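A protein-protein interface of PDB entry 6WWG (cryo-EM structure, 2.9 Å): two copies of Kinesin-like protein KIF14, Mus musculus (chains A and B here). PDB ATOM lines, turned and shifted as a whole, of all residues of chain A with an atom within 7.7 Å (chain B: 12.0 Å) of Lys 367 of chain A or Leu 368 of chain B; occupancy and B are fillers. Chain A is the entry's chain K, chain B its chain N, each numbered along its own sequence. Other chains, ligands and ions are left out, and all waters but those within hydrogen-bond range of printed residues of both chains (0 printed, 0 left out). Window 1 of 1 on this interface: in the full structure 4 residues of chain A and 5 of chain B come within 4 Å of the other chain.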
ATOM      1  N   ASP A 245      13.379   5.252   7.108  1.00  0.00           N
ATOM      2  CA  ASP A 245      13.712   6.582   7.604  1.00  0.00           C
ATOM      3  C   ASP A 245      13.022   6.930   8.919  1.00  0.00           C
ATOM      4  O   ASP A 245      12.855   8.119   9.211  1.00  0.00           O
ATOM      5  CB  ASP A 245      13.367   7.628   6.535  1.00  0.00           C
ATOM      6  CG  ASP A 245      14.286   7.554   5.324  1.00  0.00           C
ATOM      7  OD1 ASP A 245      15.463   7.163   5.484  1.00  0.00           O
ATOM      8  OD2 ASP A 245      13.832   7.890   4.212  1.00  0.00           O
ATOM      9  N   GLU A 362      11.568   9.452  18.884  1.00  0.00           N
ATOM     10  CA  GLU A 362      11.434   9.368  17.436  1.00  0.00           C
ATOM     11  C   GLU A 362      12.738   9.675  16.711  1.00  0.00           C
ATOM     12  O   GLU A 362      12.848   9.379  15.517  1.00  0.00           O
ATOM     13  CB  GLU A 362      10.334  10.313  16.954  1.00  0.00           C
ATOM     14  CG  GLU A 362       8.937   9.898  17.384  1.00  0.00           C
ATOM     15  CD  GLU A 362       7.888  10.178  16.325  1.00  0.00           C
ATOM     16  OE1 GLU A 362       7.239   9.215  15.863  1.00  0.00           O
ATOM     17  OE2 GLU A 362       7.713  11.356  15.954  1.00  0.00           O
ATOM     18  N   ASP A 363      13.721  10.261  17.396  1.00  0.00           N
ATOM     19  CA  ASP A 363      15.024  10.550  16.799  1.00  0.00           C
ATOM     20  C   ASP A 363      14.885  11.543  15.646  1.00  0.00           C
ATOM     21  O   ASP A 363      15.607  11.470  14.649  1.00  0.00           O
ATOM     22  CB  ASP A 363      15.703   9.259  16.331  1.00  0.00           C
ATOM     23  CG  ASP A 363      17.205   9.404  16.184  1.00  0.00           C
ATOM     24  OD1 ASP A 363      17.696  10.550  16.123  1.00  0.00           O
ATOM     25  OD2 ASP A 363      17.896   8.365  16.129  1.00  0.00           O
ATOM     26  N   MET A 364      13.938  12.482  15.785  1.00  0.00           N
ATOM     27  CA  MET A 364      13.629  13.434  14.725  1.00  0.00           C
ATOM     28  C   MET A 364      13.359  14.847  15.230  1.00  0.00           C
ATOM     29  O   MET A 364      13.103  15.735  14.409  1.00  0.00           O
ATOM     30  CB  MET A 364      12.409  12.922  13.926  1.00  0.00           C
ATOM     31  CG  MET A 364      12.041  13.688  12.648  1.00  0.00           C
ATOM     32  SD  MET A 364      13.403  13.974  11.504  1.00  0.00           S
ATOM     33  CE  MET A 364      13.463  12.394  10.666  1.00  0.00           C
ATOM     34  N   ASN A 365      13.448  15.103  16.533  1.00  0.00           N
ATOM     35  CA  ASN A 365      13.115  16.423  17.054  1.00  0.00           C
ATOM     36  C   ASN A 365      14.135  17.461  16.597  1.00  0.00           C
ATOM     37  O   ASN A 365      15.341  17.198  16.564  1.00  0.00           O
ATOM     38  CB  ASN A 365      13.032  16.388  18.581  1.00  0.00           C
ATOM     39  CG  ASN A 365      11.815  15.626  19.081  1.00  0.00           C
ATOM     40  OD1 ASN A 365      10.993  15.158  18.291  1.00  0.00           O
ATOM     41  ND2 ASN A 365      11.688  15.511  20.398  1.00  0.00           N
ATOM     42  N   ALA A 366      13.631  18.637  16.227  1.00  0.00           N
ATOM     43  CA  ALA A 366      14.348  19.807  15.723  1.00  0.00           C
ATOM     44  C   ALA A 366      14.795  19.641  14.274  1.00  0.00           C
ATOM     45  O   ALA A 366      15.288  20.616  13.692  1.00  0.00           O
ATOM     46  CB  ALA A 366      15.580  20.165  16.573  1.00  0.00           C
ATOM     47  N   LYS A 367      14.648  18.461  13.670  1.00  0.00           N
ATOM     48  CA  LYS A 367      15.256  18.213  12.357  1.00  0.00           C
ATOM     49  C   LYS A 367      14.359  18.638  11.194  1.00  0.00           C
ATOM     50  O   LYS A 367      14.648  19.629  10.518  1.00  0.00           O
ATOM     51  CB  LYS A 367      15.637  16.733  12.270  1.00  0.00           C
ATOM     52  CG  LYS A 367      17.057  16.459  12.775  1.00  0.00           C
ATOM     53  CD  LYS A 367      17.212  15.056  13.345  1.00  0.00           C
ATOM     54  CE  LYS A 367      17.115  13.973  12.286  1.00  0.00           C
ATOM     55  NZ  LYS A 367      17.205  12.615  12.886  1.00  0.00           N
ATOM     56  N   LEU A 368      13.275  17.893  10.939  1.00  0.00           N
ATOM     57  CA  LEU A 368      12.342  18.247   9.865  1.00  0.00           C
ATOM     58  C   LEU A 368      10.880  18.028  10.249  1.00  0.00           C
ATOM     59  O   LEU A 368      10.003  18.873  10.009  1.00  0.00           O
ATOM     60  CB  LEU A 368      12.682  17.432   8.613  1.00  0.00           C
ATOM     61  CG  LEU A 368      11.884  17.662   7.329  1.00  0.00           C
ATOM     62  CD1 LEU A 368      12.158  19.050   6.772  1.00  0.00           C
ATOM     63  CD2 LEU A 368      12.239  16.585   6.315  1.00  0.00           C
ATOM     64  N   ILE A 369      10.605  16.893  10.884  1.00  0.00           N
ATOM     65  CA  ILE A 369       9.227  16.523  11.171  1.00  0.00           C
ATOM     66  C   ILE A 369       8.755  17.137  12.477  1.00  0.00           C
ATOM     67  O   ILE A 369       7.541  17.179  12.728  1.00  0.00           O
ATOM     68  CB  ILE A 369       9.050  14.988  11.171  1.00  0.00           C
ATOM     69  CG1 ILE A 369       9.610  14.370   9.873  1.00  0.00           C
ATOM     70  CG2 ILE A 369       7.596  14.619  11.353  1.00  0.00           C
ATOM     71  CD1 ILE A 369       9.034  14.922   8.567  1.00  0.00           C
ATOM     72  N   ARG A 370       9.673  17.645  13.303  1.00  0.00           N
ATOM     73  CA  ARG A 370       9.286  18.520  14.402  1.00  0.00           C
ATOM     74  C   ARG A 370       8.568  19.753  13.880  1.00  0.00           C
ATOM     75  O   ARG A 370       7.562  20.185  14.454  1.00  0.00           O
ATOM     76  CB  ARG A 370      10.533  18.919  15.189  1.00  0.00           C
ATOM     77  CG  ARG A 370      10.338  19.893  16.365  1.00  0.00           C
ATOM     78  CD  ARG A 370       9.709  19.231  17.577  1.00  0.00           C
ATOM     79  NE  ARG A 370       8.253  19.193  17.489  1.00  0.00           N
ATOM     80  CZ  ARG A 370       7.460  18.537  18.333  1.00  0.00           C
ATOM     81  NH1 ARG A 370       7.968  17.854  19.356  1.00  0.00           N
ATOM     82  NH2 ARG A 370       6.148  18.567  18.155  1.00  0.00           N
ATOM     83  N   GLU A 371       9.071  20.333  12.791  1.00  0.00           N
ATOM     84  CA  GLU A 371       8.439  21.497  12.189  1.00  0.00           C
ATOM     85  C   GLU A 371       7.274  21.116  11.287  1.00  0.00           C
ATOM     86  O   GLU A 371       6.368  21.935  11.098  1.00  0.00           O
ATOM     87  CB  GLU A 371       9.475  22.312  11.412  1.00  0.00           C
ATOM     88  CG  GLU A 371      10.461  23.066  12.308  1.00  0.00           C
ATOM     89  CD  GLU A 371      11.558  22.183  12.881  1.00  0.00           C
ATOM     90  OE1 GLU A 371      11.589  20.979  12.556  1.00  0.00           O
ATOM     91  OE2 GLU A 371      12.389  22.695  13.660  1.00  0.00           O
ATOM     92  N   LEU A 372       7.277  19.904  10.719  1.00  0.00           N
ATOM     93  CA  LEU A 372       6.032  19.355  10.180  1.00  0.00           C
ATOM     94  C   LEU A 372       4.941  19.402  11.239  1.00  0.00           C
ATOM     95  O   LEU A 372       3.840  19.912  10.999  1.00  0.00           O
ATOM     96  CB  LEU A 372       6.219  17.903   9.715  1.00  0.00           C
ATOM     97  CG  LEU A 372       5.019  17.270   8.983  1.00  0.00           C
ATOM     98  CD1 LEU A 372       4.862  17.855   7.590  1.00  0.00           C
ATOM     99  CD2 LEU A 372       5.061  15.752   8.888  1.00  0.00           C
ATOM    100  N   LYS B 359      29.108  26.400   5.633  1.00  0.00           N
ATOM    101  CA  LYS B 359      28.805  24.972   5.597  1.00  0.00           C
ATOM    102  C   LYS B 359      27.290  24.789   5.592  1.00  0.00           C
ATOM    103  O   LYS B 359      26.657  24.435   6.590  1.00  0.00           O
ATOM    104  CB  LYS B 359      29.481  24.251   6.756  1.00  0.00           C
ATOM    105  CG  LYS B 359      30.994  24.201   6.598  1.00  0.00           C
ATOM    106  CD  LYS B 359      31.665  23.245   7.574  1.00  0.00           C
ATOM    107  CE  LYS B 359      31.768  23.821   8.974  1.00  0.00           C
ATOM    108  NZ  LYS B 359      32.554  22.921   9.864  1.00  0.00           N
ATOM    109  N   VAL B 360      26.709  25.043   4.420  1.00  0.00           N
ATOM    110  CA  VAL B 360      25.319  24.721   4.114  1.00  0.00           C
ATOM    111  C   VAL B 360      25.207  23.417   3.335  1.00  0.00           C
ATOM    112  O   VAL B 360      24.088  22.933   3.104  1.00  0.00           O
ATOM    113  CB  VAL B 360      24.644  25.881   3.345  1.00  0.00           C
ATOM    114  CG1 VAL B 360      23.164  25.593   3.044  1.00  0.00           C
ATOM    115  CG2 VAL B 360      24.776  27.190   4.122  1.00  0.00           C
ATOM    116  N   ASN B 361      26.341  22.807   2.961  1.00  0.00           N
ATOM    117  CA  ASN B 361      26.331  21.562   2.199  1.00  0.00           C
ATOM    118  C   ASN B 361      25.524  20.475   2.895  1.00  0.00           C
ATOM    119  O   ASN B 361      24.919  19.628   2.225  1.00  0.00           O
ATOM    120  CB  ASN B 361      27.765  21.078   1.982  1.00  0.00           C
ATOM    121  CG  ASN B 361      28.535  21.953   1.010  1.00  0.00           C
ATOM    122  OD1 ASN B 361      28.310  23.160   0.932  1.00  0.00           O
ATOM    123  ND2 ASN B 361      29.463  21.349   0.273  1.00  0.00           N
ATOM    124  N   GLU B 362      25.512  20.472   4.228  1.00  0.00           N
ATOM    125  CA  GLU B 362      24.729  19.526   5.020  1.00  0.00           C
ATOM    126  C   GLU B 362      23.941  20.310   6.064  1.00  0.00           C
ATOM    127  O   GLU B 362      24.394  20.475   7.201  1.00  0.00           O
ATOM    128  CB  GLU B 362      25.636  18.478   5.667  1.00  0.00           C
ATOM    129  CG  GLU B 362      24.908  17.434   6.512  1.00  0.00           C
ATOM    130  CD  GLU B 362      23.964  16.571   5.698  1.00  0.00           C
ATOM    131  OE1 GLU B 362      24.197  16.417   4.481  1.00  0.00           O
ATOM    132  OE2 GLU B 362      22.990  16.045   6.276  1.00  0.00           O
ATOM    133  N   ASP B 363      22.763  20.789   5.679  1.00  0.00           N
ATOM    134  CA  ASP B 363      21.747  21.105   6.670  1.00  0.00           C
ATOM    135  C   ASP B 363      21.220  19.788   7.223  1.00  0.00           C
ATOM    136  O   ASP B 363      21.007  18.835   6.469  1.00  0.00           O
ATOM    137  CB  ASP B 363      20.626  21.942   6.052  1.00  0.00           C
ATOM    138  CG  ASP B 363      21.079  23.347   5.684  1.00  0.00           C
ATOM    139  OD1 ASP B 363      22.006  23.869   6.338  1.00  0.00           O
ATOM    140  OD2 ASP B 363      20.503  23.932   4.742  1.00  0.00           O
ATOM    141  N   MET B 364      21.025  19.739   8.542  1.00  0.00           N
ATOM    142  CA  MET B 364      20.986  18.474   9.272  1.00  0.00           C
ATOM    143  C   MET B 364      19.967  17.476   8.727  1.00  0.00           C
ATOM    144  O   MET B 364      20.242  16.272   8.666  1.00  0.00           O
ATOM    145  CB  MET B 364      20.721  18.752  10.754  1.00  0.00           C
ATOM    146  CG  MET B 364      21.834  19.550  11.427  1.00  0.00           C
ATOM    147  SD  MET B 364      23.411  18.673  11.458  1.00  0.00           S
ATOM    148  CE  MET B 364      24.514  19.982  11.975  1.00  0.00           C
ATOM    149  N   ASN B 365      18.782  17.948   8.334  1.00  0.00           N
ATOM    150  CA  ASN B 365      17.727  17.057   7.835  1.00  0.00           C
ATOM    151  C   ASN B 365      16.978  17.759   6.704  1.00  0.00           C
ATOM    152  O   ASN B 365      15.959  18.416   6.936  1.00  0.00           O
ATOM    153  CB  ASN B 365      16.786  16.644   8.955  1.00  0.00           C
ATOM    154  CG  ASN B 365      15.913  15.467   8.574  1.00  0.00           C
ATOM    155  OD1 ASN B 365      14.989  15.599   7.771  1.00  0.00           O
ATOM    156  ND2 ASN B 365      16.209  14.304   9.140  1.00  0.00           N
ATOM    157  N   ALA B 366      17.491  17.594   5.484  1.00  0.00           N
ATOM    158  CA  ALA B 366      16.782  17.935   4.248  1.00  0.00           C
ATOM    159  C   ALA B 366      16.245  19.364   4.262  1.00  0.00           C
ATOM    160  O   ALA B 366      15.042  19.603   4.136  1.00  0.00           O
ATOM    161  CB  ALA B 366      15.655  16.937   3.989  1.00  0.00           C
ATOM    162  N   LYS B 367      17.159  20.327   4.393  1.00  0.00           N
ATOM    163  CA  LYS B 367      16.828  21.748   4.303  1.00  0.00           C
ATOM    164  C   LYS B 367      15.796  22.132   5.369  1.00  0.00           C
ATOM    165  O   LYS B 367      14.614  22.359   5.093  1.00  0.00           O
ATOM    166  CB  LYS B 367      16.345  22.102   2.890  1.00  0.00           C
ATOM    167  CG  LYS B 367      17.303  21.668   1.774  1.00  0.00           C
ATOM    168  CD  LYS B 367      18.699  22.277   1.923  1.00  0.00           C
ATOM    169  CE  LYS B 367      19.645  21.766   0.852  1.00  0.00           C
ATOM    170  NZ  LYS B 367      19.255  22.222  -0.502  1.00  0.00           N
ATOM    171  N   LEU B 368      16.290  22.140   6.614  1.00  0.00           N
ATOM    172  CA  LEU B 368      15.579  22.615   7.802  1.00  0.00           C
ATOM    173  C   LEU B 368      14.663  23.796   7.504  1.00  0.00           C
ATOM    174  O   LEU B 368      13.494  23.811   7.909  1.00  0.00           O
ATOM    175  CB  LEU B 368      16.582  23.052   8.877  1.00  0.00           C
ATOM    176  CG  LEU B 368      17.747  22.148   9.292  1.00  0.00           C
ATOM    177  CD1 LEU B 368      18.501  22.775  10.455  1.00  0.00           C
ATOM    178  CD2 LEU B 368      17.269  20.766   9.688  1.00  0.00           C
ATOM    179  N   ILE B 369      15.197  24.774   6.768  1.00  0.00           N
ATOM    180  CA  ILE B 369      14.495  26.024   6.525  1.00  0.00           C
ATOM    181  C   ILE B 369      13.178  25.816   5.792  1.00  0.00           C
ATOM    182  O   ILE B 369      12.234  26.577   6.021  1.00  0.00           O
ATOM    183  CB  ILE B 369      15.413  26.980   5.737  1.00  0.00           C
ATOM    184  CG1 ILE B 369      14.834  28.398   5.719  1.00  0.00           C
ATOM    185  CG2 ILE B 369      15.633  26.471   4.310  1.00  0.00           C
ATOM    186  CD1 ILE B 369      15.825  29.447   5.262  1.00  0.00           C
ATOM    187  N   ARG B 370      13.080  24.784   4.943  1.00  0.00           N
ATOM    188  CA  ARG B 370      11.891  24.597   4.115  1.00  0.00           C
ATOM    189  C   ARG B 370      10.621  24.490   4.949  1.00  0.00           C
ATOM    190  O   ARG B 370       9.543  24.884   4.487  1.00  0.00           O
ATOM    191  CB  ARG B 370      12.046  23.348   3.244  1.00  0.00           C
ATOM    192  CG  ARG B 370      10.874  23.096   2.295  1.00  0.00           C
ATOM    193  CD  ARG B 370      11.140  21.904   1.401  1.00  0.00           C
ATOM    194  NE  ARG B 370      10.034  21.643   0.481  1.00  0.00           N
ATOM    195  CZ  ARG B 370       8.868  21.103   0.827  1.00  0.00           C
ATOM    196  NH1 ARG B 370       8.619  20.752   2.084  1.00  0.00           N
ATOM    197  NH2 ARG B 370       7.936  20.914  -0.097  1.00  0.00           N
ATOM    198  N   GLU B 371      10.725  23.961   6.172  1.00  0.00           N
ATOM    199  CA  GLU B 371       9.592  23.851   7.079  1.00  0.00           C
ATOM    200  C   GLU B 371       9.752  24.644   8.367  1.00  0.00           C
ATOM    201  O   GLU B 371       8.743  24.908   9.029  1.00  0.00           O
ATOM    202  CB  GLU B 371       9.328  22.377   7.429  1.00  0.00           C
ATOM    203  CG  GLU B 371       8.831  21.546   6.249  1.00  0.00           C
ATOM    204  CD  GLU B 371       7.453  21.970   5.772  1.00  0.00           C
ATOM    205  OE1 GLU B 371       6.655  22.450   6.605  1.00  0.00           O
ATOM    206  OE2 GLU B 371       7.168  21.822   4.565  1.00  0.00           O
ATOM    207  N   LEU B 372      10.974  25.036   8.741  1.00  0.00           N
ATOM    208  CA  LEU B 372      11.141  25.923   9.887  1.00  0.00           C
ATOM    209  C   LEU B 372      10.798  27.369   9.550  1.00  0.00           C
ATOM    210  O   LEU B 372      10.502  28.147  10.465  1.00  0.00           O
ATOM    211  CB  LEU B 372      12.575  25.807  10.419  1.00  0.00           C
ATOM    212  CG  LEU B 372      12.901  26.446  11.774  1.00  0.00           C
ATOM    213  CD1 LEU B 372      13.886  25.565  12.522  1.00  0.00           C
ATOM    214  CD2 LEU B 372      13.491  27.839  11.626  1.00  0.00           C
ATOM    215  N   LYS B 373      10.809  27.739   8.270  1.00  0.00           N
ATOM    216  CA  LYS B 373      10.451  29.086   7.828  1.00  0.00           C
ATOM    217  C   LYS B 373       9.076  29.512   8.334  1.00  0.00           C
ATOM    218  O   LYS B 373       8.952  30.491   9.070  1.00  0.00           O
ATOM    219  CB  LYS B 373      10.482  29.156   6.300  1.00  0.00           C
ATOM    220  CG  LYS B 373      10.207  30.530   5.723  1.00  0.00           C
ATOM    221  CD  LYS B 373      10.633  30.590   4.269  1.00  0.00           C
ATOM    222  CE  LYS B 373      10.157  31.862   3.598  1.00  0.00           C
ATOM    223  NZ  LYS B 373       9.024  31.609   2.666  1.00  0.00           N
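Lys 367 of chain A touches Asn 365 of chain B (CE to ND2, 3.3 Å). Lys 367 of chain A touches Leu 368 of chain B. Leu 368 of chain A touches Asn 365 of chain B. Leu 368 of chain A touches Ala 366 of chain B. Glu 371 of chain A touches Glu 371 of chain B. Leu 372 of chain B touches Glu 371 of chain A.
Met 364 of chain A touches just one residue of chain B: Asn 365. Asn 365 of chain A touches none of the printed residues of chain B. No residue of chain B comes within 4 Å of Ala 366 of chain A. Lys 367 of chain A touches just these residues of chain B: Asn 365 (3.3 Å) and Leu 368 (3.0 Å). Of chain B, only Asn 365 (3.1 Å) and Ala 366 (3.9 Å) come within 4 Å of Leu 368 of chain A. Arg 370 of chain A touches none of the printed residues of chain B. Of the printed residues of chain B, Glu 371 of chain A touches Glu 371 (3.6 Å) and Leu 372 (3.4 Å). Printed residues of chain A within 4 Å of Asn 365 of chain B: Met 364 (3.7 Å), Lys 367 (3.3 Å) and Leu 368 (3.1 Å). Printed residues of chain A within 4 Å of Ala 366 of chain B: Leu 368 (3.9 Å). Of the printed residues of chain A, Leu 368 of chain B touches Lys 367. Printed residues of chain A within 4 Å of Glu 371 of chain B: Glu 371 (3.6 Å). Of the printed residues of chain A, Leu 372 of chain B touches Glu 371.
Printed residues of chain B that touch a printed residue of chain A: Asn 365, Ala 366, Leu 368, Glu 371 and Leu 372. Hydrophobic or aromatic side chains of chain B within 4 Å of the printed part of chain A: Leu 368 and Leu 372. Printed residues of chain A that touch a printed residue of chain B: Met 364, Lys 367, Leu 368 and Glu 371. Among the printed residues, no Asp or Glu carboxylate lies within 4 Å of a Lys or Arg side-chain nitrogen of the other chain.
The side-chain carboxylate (OD1) of Asp 363 of chain A lies within salt-bridge range of the side-chain amino group (NZ) of Lys 367 of chain A, at 3.9 Å. The guanidinium group of Arg 370 of chain B lies within salt-bridge range of the side-chain carboxylate of Glu 371 of chain B, at 3.1 Å.
The side-chain sulfur (SD) of Met 364 of chain A sits close to the side-chain amide nitrogen (ND2) of Asn 365 of chain B, at 3.7 Å.
Lys 367 of chain A touches Asn 365 of chain B, but with the chains exchanged Asn 365 of chain A does not touch Lys 367 of chain B (12.2 Å). Lys 367 of chain A touches Leu 368 of chain B, but with the chains exchanged Leu 368 of chain A does not touch Lys 367 of chain B (4.4 Å). Leu 368 of chain A touches Asn 365 of chain B, but with the chains exchanged Asn 365 of chain A does not touch Leu 368 of chain B (8.0 Å). Glu 371 of chain A touches Leu 372 of chain B, but with the chains exchanged Leu 372 of chain A does not touch Glu 371 of chain B (4.6 Å). Positions printed for both chains: 362, 363, 364, 365, 366, 367, 368, 369, 370, 371 and 372.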
